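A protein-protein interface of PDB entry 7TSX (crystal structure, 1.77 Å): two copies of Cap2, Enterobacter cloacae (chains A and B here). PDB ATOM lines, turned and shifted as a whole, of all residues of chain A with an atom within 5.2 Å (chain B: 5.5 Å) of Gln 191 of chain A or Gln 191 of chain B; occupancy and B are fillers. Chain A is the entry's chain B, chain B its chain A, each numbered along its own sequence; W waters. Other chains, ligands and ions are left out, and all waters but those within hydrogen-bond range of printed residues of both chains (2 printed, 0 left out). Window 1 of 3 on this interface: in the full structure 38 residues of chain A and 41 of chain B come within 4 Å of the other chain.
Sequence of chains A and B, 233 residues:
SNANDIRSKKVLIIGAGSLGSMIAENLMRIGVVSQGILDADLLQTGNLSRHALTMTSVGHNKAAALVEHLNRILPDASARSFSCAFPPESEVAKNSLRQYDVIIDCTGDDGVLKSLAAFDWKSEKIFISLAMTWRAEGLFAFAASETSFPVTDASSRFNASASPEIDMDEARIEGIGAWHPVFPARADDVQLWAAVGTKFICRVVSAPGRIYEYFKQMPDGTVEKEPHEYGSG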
ATOM      1  N   MET A  22     -27.078 -18.577  18.782  1.00  0.00           N
ATOM      2  CA  MET A  22     -26.770 -17.445  17.915  1.00  0.00           C
ATOM      3  C   MET A  22     -28.014 -16.928  17.206  1.00  0.00           C
ATOM      4  O   MET A  22     -28.186 -15.704  17.049  1.00  0.00           O
ATOM      5  CB  MET A  22     -25.705 -17.838  16.901  1.00  0.00           C
ATOM      6  CG  MET A  22     -24.370 -18.143  17.518  1.00  0.00           C
ATOM      7  SD  MET A  22     -23.142 -18.546  16.256  1.00  0.00           S
ATOM      8  CE  MET A  22     -21.828 -19.240  17.254  1.00  0.00           C
ATOM      9  N   ASN A  26     -29.708 -13.143  17.540  1.00  0.00           N
ATOM     10  CA  ASN A  26     -30.045 -12.312  16.387  1.00  0.00           C
ATOM     11  C   ASN A  26     -31.509 -11.882  16.445  1.00  0.00           C
ATOM     12  O   ASN A  26     -31.844 -10.712  16.221  1.00  0.00           O
ATOM     13  CB  ASN A  26     -29.782 -13.054  15.071  1.00  0.00           C
ATOM     14  CG  ASN A  26     -28.314 -13.289  14.799  1.00  0.00           C
ATOM     15  OD1 ASN A  26     -27.443 -12.692  15.420  1.00  0.00           O
ATOM     16  ND2 ASN A  26     -28.033 -14.158  13.824  1.00  0.00           N
ATOM     17  N   ARG A 186     -16.031 -23.611  12.815  1.00  0.00           N
ATOM     18  CA  ARG A 186     -15.546 -22.524  13.656  1.00  0.00           C
ATOM     19  C   ARG A 186     -16.667 -21.527  13.931  1.00  0.00           C
ATOM     20  O   ARG A 186     -17.759 -21.601  13.368  1.00  0.00           O
ATOM     21  CB  ARG A 186     -14.367 -21.797  12.998  1.00  0.00           C
ATOM     22  CG  ARG A 186     -13.268 -22.698  12.486  1.00  0.00           C
ATOM     23  CD  ARG A 186     -12.040 -21.897  12.044  1.00  0.00           C
ATOM     24  NE  ARG A 186     -12.399 -20.730  11.240  1.00  0.00           N
ATOM     25  CZ  ARG A 186     -11.533 -20.014  10.535  1.00  0.00           C
ATOM     26  NH1 ARG A 186     -10.255 -20.352  10.464  1.00  0.00           N
ATOM     27  NH2 ARG A 186     -11.958 -18.927   9.889  1.00  0.00           N
ATOM     28  N   ALA A 187     -16.374 -20.562  14.800  1.00  0.00           N
ATOM     29  CA  ALA A 187     -17.383 -19.568  15.148  1.00  0.00           C
ATOM     30  C   ALA A 187     -17.877 -18.834  13.914  1.00  0.00           C
ATOM     31  O   ALA A 187     -19.073 -18.545  13.793  1.00  0.00           O
ATOM     32  CB  ALA A 187     -16.813 -18.579  16.170  1.00  0.00           C
ATOM     33  N   ASP A 188     -16.970 -18.493  12.995  1.00  0.00           N
ATOM     34  CA  ASP A 188     -17.395 -17.749  11.810  1.00  0.00           C
ATOM     35  C   ASP A 188     -18.304 -18.580  10.912  1.00  0.00           C
ATOM     36  O   ASP A 188     -19.201 -18.031  10.257  1.00  0.00           O
ATOM     37  CB  ASP A 188     -16.186 -17.267  11.013  1.00  0.00           C
ATOM     38  CG  ASP A 188     -15.186 -18.362  10.739  1.00  0.00           C
ATOM     39  OD1 ASP A 188     -14.715 -19.002  11.702  1.00  0.00           O
ATOM     40  OD2 ASP A 188     -14.866 -18.591   9.557  1.00  0.00           O
ATOM     41  N   ASP A 189     -18.086 -19.895  10.858  1.00  0.00           N
ATOM     42  CA  ASP A 189     -18.985 -20.759  10.092  1.00  0.00           C
ATOM     43  C   ASP A 189     -20.390 -20.748  10.681  1.00  0.00           C
ATOM     44  O   ASP A 189     -21.387 -20.647   9.954  1.00  0.00           O
ATOM     45  CB  ASP A 189     -18.455 -22.195  10.060  1.00  0.00           C
ATOM     46  CG  ASP A 189     -17.130 -22.326   9.356  1.00  0.00           C
ATOM     47  OD1 ASP A 189     -17.007 -21.911   8.176  1.00  0.00           O
ATOM     48  OD2 ASP A 189     -16.203 -22.887   9.990  1.00  0.00           O
ATOM     49  N   VAL A 190     -20.492 -20.894  12.002  1.00  0.00           N
ATOM     50  CA  VAL A 190     -21.798 -20.990  12.629  1.00  0.00           C
ATOM     51  C   VAL A 190     -22.500 -19.642  12.620  1.00  0.00           C
ATOM     52  O   VAL A 190     -23.721 -19.575  12.452  1.00  0.00           O
ATOM     53  CB  VAL A 190     -21.673 -21.547  14.057  1.00  0.00           C
ATOM     54  CG1 VAL A 190     -23.049 -21.679  14.711  1.00  0.00           C
ATOM     55  CG2 VAL A 190     -20.953 -22.885  14.041  1.00  0.00           C
ATOM     56  N   GLN A 191     -21.753 -18.549  12.826  1.00  0.00           N
ATOM     57  CA  GLN A 191     -22.371 -17.231  12.769  1.00  0.00           C
ATOM     58  C   GLN A 191     -22.907 -16.967  11.372  1.00  0.00           C
ATOM     59  O   GLN A 191     -23.952 -16.339  11.208  1.00  0.00           O
ATOM     60  CB  GLN A 191     -21.373 -16.136  13.161  1.00  0.00           C
ATOM     61  CG  GLN A 191     -21.047 -16.064  14.647  1.00  0.00           C
ATOM     62  CD  GLN A 191     -22.142 -15.419  15.486  1.00  0.00           C
ATOM     63  OE1 GLN A 191     -23.249 -15.136  15.012  1.00  0.00           O
ATOM     64  NE2 GLN A 191     -21.842 -15.209  16.757  1.00  0.00           N
ATOM     65  N   LEU A 192     -22.183 -17.421  10.351  1.00  0.00           N
ATOM     66  CA  LEU A 192     -22.671 -17.302   8.983  1.00  0.00           C
ATOM     67  C   LEU A 192     -24.021 -17.991   8.835  1.00  0.00           C
ATOM     68  O   LEU A 192     -24.970 -17.414   8.295  1.00  0.00           O
ATOM     69  CB  LEU A 192     -21.649 -17.899   8.017  1.00  0.00           C
ATOM     70  CG  LEU A 192     -21.995 -17.766   6.529  1.00  0.00           C
ATOM     71  CD1 LEU A 192     -21.611 -16.383   6.043  1.00  0.00           C
ATOM     72  CD2 LEU A 192     -21.281 -18.845   5.719  1.00  0.00           C
ATOM     73  N   TRP A 193     -24.137 -19.222   9.337  1.00  0.00           N
ATOM     74  CA  TRP A 193     -25.393 -19.953   9.177  1.00  0.00           C
ATOM     75  C   TRP A 193     -26.479 -19.428  10.116  1.00  0.00           C
ATOM     76  O   TRP A 193     -27.666 -19.467   9.775  1.00  0.00           O
ATOM     77  CB  TRP A 193     -25.159 -21.452   9.378  1.00  0.00           C
ATOM     78  CG  TRP A 193     -24.375 -22.098   8.290  1.00  0.00           C
ATOM     79  CD1 TRP A 193     -23.349 -22.982   8.448  1.00  0.00           C
ATOM     80  CD2 TRP A 193     -24.553 -21.943   6.861  1.00  0.00           C
ATOM     81  NE1 TRP A 193     -22.876 -23.376   7.220  1.00  0.00           N
ATOM     82  CE2 TRP A 193     -23.596 -22.753   6.233  1.00  0.00           C
ATOM     83  CE3 TRP A 193     -25.424 -21.201   6.068  1.00  0.00           C
ATOM     84  CZ2 TRP A 193     -23.477 -22.831   4.847  1.00  0.00           C
ATOM     85  CZ3 TRP A 193     -25.300 -21.261   4.704  1.00  0.00           C
ATOM     86  CH2 TRP A 193     -24.339 -22.082   4.100  1.00  0.00           C
ATOM     87  N   ALA A 194     -26.103 -18.890  11.275  1.00  0.00           N
ATOM     88  CA  ALA A 194     -27.102 -18.251  12.126  1.00  0.00           C
ATOM     89  C   ALA A 194     -27.685 -17.019  11.451  1.00  0.00           C
ATOM     90  O   ALA A 194     -28.869 -16.711  11.621  1.00  0.00           O
ATOM     91  CB  ALA A 194     -26.479 -17.870  13.481  1.00  0.00           C
ATOM     92  N   ALA A 195     -26.867 -16.300  10.683  1.00  0.00           N
ATOM     93  CA  ALA A 195     -27.362 -15.131   9.965  1.00  0.00           C
ATOM     94  C   ALA A 195     -28.251 -15.547   8.798  1.00  0.00           C
ATOM     95  O   ALA A 195     -29.358 -15.022   8.613  1.00  0.00           O
ATOM     96  CB  ALA A 195     -26.188 -14.284   9.476  1.00  0.00           C
ATOM     97  N   VAL A 196     -27.771 -16.478   7.980  1.00  0.00           N
ATOM     98  CA  VAL A 196     -28.601 -17.004   6.898  1.00  0.00           C
ATOM     99  C   VAL A 196     -29.888 -17.581   7.461  1.00  0.00           C
ATOM    100  O   VAL A 196     -30.978 -17.367   6.912  1.00  0.00           O
ATOM    101  CB  VAL A 196     -27.817 -18.058   6.096  1.00  0.00           C
ATOM    102  CG1 VAL A 196     -28.725 -18.735   5.076  1.00  0.00           C
ATOM    103  CG2 VAL A 196     -26.619 -17.411   5.405  1.00  0.00           C
ATOM    104  N   MET B  22     -18.251  -7.656  16.439  1.00  0.00           N
ATOM    105  CA  MET B  22     -18.588  -9.030  16.074  1.00  0.00           C
ATOM    106  C   MET B  22     -17.390  -9.765  15.490  1.00  0.00           C
ATOM    107  O   MET B  22     -17.192 -10.956  15.757  1.00  0.00           O
ATOM    108  CB  MET B  22     -19.740  -9.032  15.080  1.00  0.00           C
ATOM    109  CG  MET B  22     -21.024  -8.463  15.676  1.00  0.00           C
ATOM    110  SD  MET B  22     -22.405  -8.592  14.545  1.00  0.00           S
ATOM    111  CE  MET B  22     -23.601  -7.548  15.370  1.00  0.00           C
ATOM    112  N   GLU B  25     -15.098 -10.761  18.351  1.00  0.00           N
ATOM    113  CA  GLU B  25     -15.573 -11.945  19.057  1.00  0.00           C
ATOM    114  C   GLU B  25     -15.307 -13.201  18.243  1.00  0.00           C
ATOM    115  O   GLU B  25     -14.876 -14.223  18.789  1.00  0.00           O
ATOM    116  CB  GLU B  25     -17.065 -11.839  19.379  1.00  0.00           C
ATOM    117  CG  GLU B  25     -17.574 -13.042  20.176  1.00  0.00           C
ATOM    118  CD  GLU B  25     -19.059 -13.014  20.434  1.00  0.00           C
ATOM    119  OE1 GLU B  25     -19.563 -11.987  20.921  1.00  0.00           O
ATOM    120  OE2 GLU B  25     -19.721 -14.024  20.114  1.00  0.00           O
ATOM    121  N   ASN B  26     -15.596 -13.159  16.938  1.00  0.00           N
ATOM    122  CA  ASN B  26     -15.315 -14.317  16.098  1.00  0.00           C
ATOM    123  C   ASN B  26     -13.848 -14.704  16.169  1.00  0.00           C
ATOM    124  O   ASN B  26     -13.509 -15.889  16.257  1.00  0.00           O
ATOM    125  CB  ASN B  26     -15.684 -14.045  14.639  1.00  0.00           C
ATOM    126  CG  ASN B  26     -17.189 -13.958  14.416  1.00  0.00           C
ATOM    127  OD1 ASN B  26     -17.978 -14.282  15.300  1.00  0.00           O
ATOM    128  ND2 ASN B  26     -17.582 -13.471  13.251  1.00  0.00           N
ATOM    129  N   ARG B 186     -29.735  -4.806  10.000  1.00  0.00           N
ATOM    130  CA  ARG B 186     -30.112  -5.447  11.249  1.00  0.00           C
ATOM    131  C   ARG B 186     -28.946  -6.293  11.742  1.00  0.00           C
ATOM    132  O   ARG B 186     -27.915  -6.409  11.073  1.00  0.00           O
ATOM    133  CB  ARG B 186     -31.369  -6.304  11.060  1.00  0.00           C
ATOM    134  CG  ARG B 186     -32.482  -5.623  10.318  1.00  0.00           C
ATOM    135  CD  ARG B 186     -33.759  -6.493  10.276  1.00  0.00           C
ATOM    136  NE  ARG B 186     -33.484  -7.859   9.844  1.00  0.00           N
ATOM    137  CZ  ARG B 186     -34.418  -8.756   9.556  1.00  0.00           C
ATOM    138  NH1 ARG B 186     -35.705  -8.454   9.621  1.00  0.00           N
ATOM    139  NH2 ARG B 186     -34.053  -9.987   9.201  1.00  0.00           N
ATOM    140  N   ALA B 187     -29.121  -6.881  12.931  1.00  0.00           N
ATOM    141  CA  ALA B 187     -28.058  -7.678  13.523  1.00  0.00           C
ATOM    142  C   ALA B 187     -27.653  -8.816  12.601  1.00  0.00           C
ATOM    143  O   ALA B 187     -26.460  -9.131  12.491  1.00  0.00           O
ATOM    144  CB  ALA B 187     -28.492  -8.219  14.892  1.00  0.00           C
ATOM    145  N   ASP B 188     -28.624  -9.452  11.937  1.00  0.00           N
ATOM    146  CA  ASP B 188     -28.280 -10.591  11.084  1.00  0.00           C
ATOM    147  C   ASP B 188     -27.415 -10.142   9.910  1.00  0.00           C
ATOM    148  O   ASP B 188     -26.517 -10.869   9.470  1.00  0.00           O
ATOM    149  CB  ASP B 188     -29.542 -11.305  10.598  1.00  0.00           C
ATOM    150  CG  ASP B 188     -30.578 -10.349   9.999  1.00  0.00           C
ATOM    151  OD1 ASP B 188     -30.948  -9.359  10.656  1.00  0.00           O
ATOM    152  OD2 ASP B 188     -31.032 -10.597   8.875  1.00  0.00           O
ATOM    153  N   ASP B 189     -27.666  -8.937   9.392  1.00  0.00           N
ATOM    154  CA  ASP B 189     -26.827  -8.398   8.326  1.00  0.00           C
ATOM    155  C   ASP B 189     -25.393  -8.212   8.797  1.00  0.00           C
ATOM    156  O   ASP B 189     -24.442  -8.587   8.102  1.00  0.00           O
ATOM    157  CB  ASP B 189     -27.374  -7.059   7.833  1.00  0.00           C
ATOM    158  CG  ASP B 189     -28.762  -7.161   7.251  1.00  0.00           C
ATOM    159  OD1 ASP B 189     -28.966  -7.957   6.306  1.00  0.00           O
ATOM    160  OD2 ASP B 189     -29.660  -6.427   7.729  1.00  0.00           O
ATOM    161  N   VAL B 190     -25.215  -7.607   9.972  1.00  0.00           N
ATOM    162  CA  VAL B 190     -23.868  -7.362  10.466  1.00  0.00           C
ATOM    163  C   VAL B 190     -23.161  -8.672  10.808  1.00  0.00           C
ATOM    164  O   VAL B 190     -21.957  -8.817  10.560  1.00  0.00           O
ATOM    165  CB  VAL B 190     -23.918  -6.420  11.674  1.00  0.00           C
ATOM    166  CG1 VAL B 190     -22.495  -6.034  12.106  1.00  0.00           C
ATOM    167  CG2 VAL B 190     -24.707  -5.174  11.332  1.00  0.00           C
ATOM    168  N   GLN B 191     -23.882  -9.634  11.403  1.00  0.00           N
ATOM    169  CA  GLN B 191     -23.272 -10.932  11.693  1.00  0.00           C
ATOM    170  C   GLN B 191     -22.837 -11.623  10.404  1.00  0.00           C
ATOM    171  O   GLN B 191     -21.760 -12.229  10.347  1.00  0.00           O
ATOM    172  CB  GLN B 191     -24.249 -11.828  12.467  1.00  0.00           C
ATOM    173  CG  GLN B 191     -24.532 -11.365  13.898  1.00  0.00           C
ATOM    174  CD  GLN B 191     -23.403 -11.712  14.872  1.00  0.00           C
ATOM    175  OE1 GLN B 191     -22.307 -12.101  14.465  1.00  0.00           O
ATOM    176  NE2 GLN B 191     -23.673 -11.573  16.165  1.00  0.00           N
ATOM    177  N   LEU B 192     -23.668 -11.552   9.355  1.00  0.00           N
ATOM    178  CA  LEU B 192     -23.275 -12.127   8.071  1.00  0.00           C
ATOM    179  C   LEU B 192     -21.934 -11.562   7.617  1.00  0.00           C
ATOM    180  O   LEU B 192     -20.999 -12.311   7.293  1.00  0.00           O
ATOM    181  CB  LEU B 192     -24.346 -11.864   7.017  1.00  0.00           C
ATOM    182  CG  LEU B 192     -24.044 -12.384   5.615  1.00  0.00           C
ATOM    183  CD1 LEU B 192     -24.133 -13.898   5.580  1.00  0.00           C
ATOM    184  CD2 LEU B 192     -25.007 -11.783   4.578  1.00  0.00           C
ATOM    185  N   TRP B 193     -21.816 -10.236   7.593  1.00  0.00           N
ATOM    186  CA  TRP B 193     -20.593  -9.626   7.082  1.00  0.00           C
ATOM    187  C   TRP B 193     -19.436  -9.751   8.067  1.00  0.00           C
ATOM    188  O   TRP B 193     -18.272  -9.751   7.651  1.00  0.00           O
ATOM    189  CB  TRP B 193     -20.846  -8.161   6.736  1.00  0.00           C
ATOM    190  CG  TRP B 193     -21.801  -7.965   5.594  1.00  0.00           C
ATOM    191  CD1 TRP B 193     -22.837  -7.073   5.536  1.00  0.00           C
ATOM    192  CD2 TRP B 193     -21.810  -8.675   4.344  1.00  0.00           C
ATOM    193  NE1 TRP B 193     -23.479  -7.178   4.326  1.00  0.00           N
ATOM    194  CE2 TRP B 193     -22.883  -8.163   3.581  1.00  0.00           C
ATOM    195  CE3 TRP B 193     -21.027  -9.705   3.801  1.00  0.00           C
ATOM    196  CZ2 TRP B 193     -23.174  -8.617   2.289  1.00  0.00           C
ATOM    197  CZ3 TRP B 193     -21.324 -10.167   2.508  1.00  0.00           C
ATOM    198  CH2 TRP B 193     -22.402  -9.634   1.781  1.00  0.00           C
ATOM    199  N   ALA B 194     -19.717  -9.831   9.371  1.00  0.00           N
ATOM    200  CA  ALA B 194     -18.643 -10.131  10.314  1.00  0.00           C
ATOM    201  C   ALA B 194     -18.087 -11.533  10.072  1.00  0.00           C
ATOM    202  O   ALA B 194     -16.888 -11.781  10.239  1.00  0.00           O
ATOM    203  CB  ALA B 194     -19.138  -9.998  11.754  1.00  0.00           C
ATOM    204  N   ALA B 195     -18.950 -12.463   9.694  1.00  0.00           N
ATOM    205  CA  ALA B 195     -18.505 -13.818   9.405  1.00  0.00           C
ATOM    206  C   ALA B 195     -17.679 -13.844   8.132  1.00  0.00           C
ATOM    207  O   ALA B 195     -16.570 -14.398   8.105  1.00  0.00           O
ATOM    208  CB  ALA B 195     -19.720 -14.748   9.291  1.00  0.00           C
ATOM    209  N   VAL B 196     -18.215 -13.253   7.061  1.00  0.00           N
ATOM    210  CA  VAL B 196     -17.474 -13.173   5.806  1.00  0.00           C
ATOM    211  C   VAL B 196     -16.173 -12.408   6.019  1.00  0.00           C
ATOM    212  O   VAL B 196     -15.116 -12.773   5.478  1.00  0.00           O
ATOM    213  CB  VAL B 196     -18.343 -12.513   4.717  1.00  0.00           C
ATOM    214  CG1 VAL B 196     -17.505 -12.216   3.476  1.00  0.00           C
ATOM    215  CG2 VAL B 196     -19.544 -13.382   4.378  1.00  0.00           C
HETATM  216  O   HOH W   1     -18.733 -15.311  17.638  1.00  0.00           O
HETATM  217  O   HOH W   2     -26.483 -10.957  17.221  1.00  0.00           O
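Water W1 lies within hydrogen-bond range of the side-chain amide oxygen (OD1) of Asn 26 of chain B (2.7 Å), the side-chain carboxylate (OE2) of Glu 25 of chain B (3.0 Å) and the side-chain amide nitrogen (NE2) of Gln 191 of chain A (3.2 Å).
Water W2 bridges the side-chain amide oxygen (OD1) of Asn 26 of chain A (2.7 Å) and the side-chain amide nitrogen (NE2) of Gln 191 of chain B (3.1 Å).
O of Met 22 of chain B sits close to OD1 of Asn 26 of chain B (3.4 Å).
The side-chain amide oxygen (OE1) of Gln 191 of chain B sits close to the side-chain sulfur (SD) of Met 22 of chain B (3.5 Å).
NE of Arg 186 of chain B is in salt-bridge range of OD1 of Asp 188 of chain B (3.1 Å).
The side-chain sulfur (SD) of Met 22 of chain A sits close to the side-chain amide nitrogen (NE2) of Gln 191 of chain A.
The side-chain amide nitrogen (ND2) of Asn 26 of chain A is in hydrogen-bond range of the backbone carbonyl oxygen (O) of Ala 194 of chain A (3.5 Å).
OD1 of Asp 188 of chain A lies within salt-bridge range of NE of Arg 186 of chain A, 2.9 Å away.
Of the 13 printed residues of chain A, 5 touch a printed residue of chain B.
Hydrophobic or aromatic side chains of chain A that line the printed part of chain B: Leu 192 and Ala 195.
Along chain A the printed residues that touch a printed residue of chain B span positions 26 to 195.
Among the printed residues, 8 pairs touch across the chains.
Among the printed residues, no Asp or Glu carboxylate lies within 4 Å of a Lys or Arg side-chain nitrogen of the other chain.
Asn 26 of chain A touches Gln 191 of chain B, and with the chains exchanged Gln 191 of chain A touches Asn 26 of chain B.
Asp 188 of chain A touches Ala 195 of chain B, and with the chains exchanged Ala 195 of chain A touches Asp 188 of chain B.
Gln 191 of chain B touches its own counterpart, Gln 191 of chain A.
Leu 192 of chain A touches its own counterpart, Leu 192 of chain B.
13 positions are printed for both chains.
Of the 8 pairs that touch across the chains among the printed residues, 8 have their exchanged pair printed and touching as well.
OE1 of Gln 191 of chain B lies close to OE1 of Gln 191 of chain A, at 3.2 Å.
Gln 191 of chain A touches just these residues of chain B: Asn 26 and Gln 191.
Gln 191 of chain B touches just these residues of chain A: Asn 26 (3.5 Å) and Gln 191 (3.2 Å).
Printed residues of chain A within 4 Å of Ala 195 of chain B: Asp 188 (3.5 Å) and Leu 192 (3.8 Å).
Printed residues of chain A within 4 Å of Asp 188 of chain B: Ala 195 (3.4 Å).
Of the printed residues of chain B, Asn 26 of chain A touches Gln 191.
Of the printed residues of chain B, Asp 188 of chain A touches Ala 195.
Of the printed residues of chain A, Asn 26 of chain B touches Gln 191 (3.6 Å).
Trp 193 of chain B touches none of the printed residues of chain A.
The nearest residue of chain B that does not touch Gln 191 of chain A is Glu 25 of chain B (4.1 Å).
The nearest residue of chain A that does not touch Gln 191 of chain B is Ala 195 of chain A (4.3 Å).
The nearest printed residue of chain B that does not touch Ala 195 of chain A is Gln 191 of chain B (4.3 Å).
OD1 of Asn 26 of chain A touches CG of Gln 191 of chain B, 3.5 Å away.
Asp 188 of chain A touches Ala 195 of chain B (O to CB, 3.5 Å).
Gln 191 of chain A touches Asn 26 of chain B (CG to OD1, 3.6 Å).
CD1 of Leu 192 of chain B touches CD1 of Leu 192 of chain A, at 3.6 Å.
Leu 192 of chain A touches Ala 195 of chain B.
Ala 195 of chain A touches Asp 188 of chain B.
N of Leu 192 of chain B touches CB of Ala 195 of chain A, 3.7 Å away.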
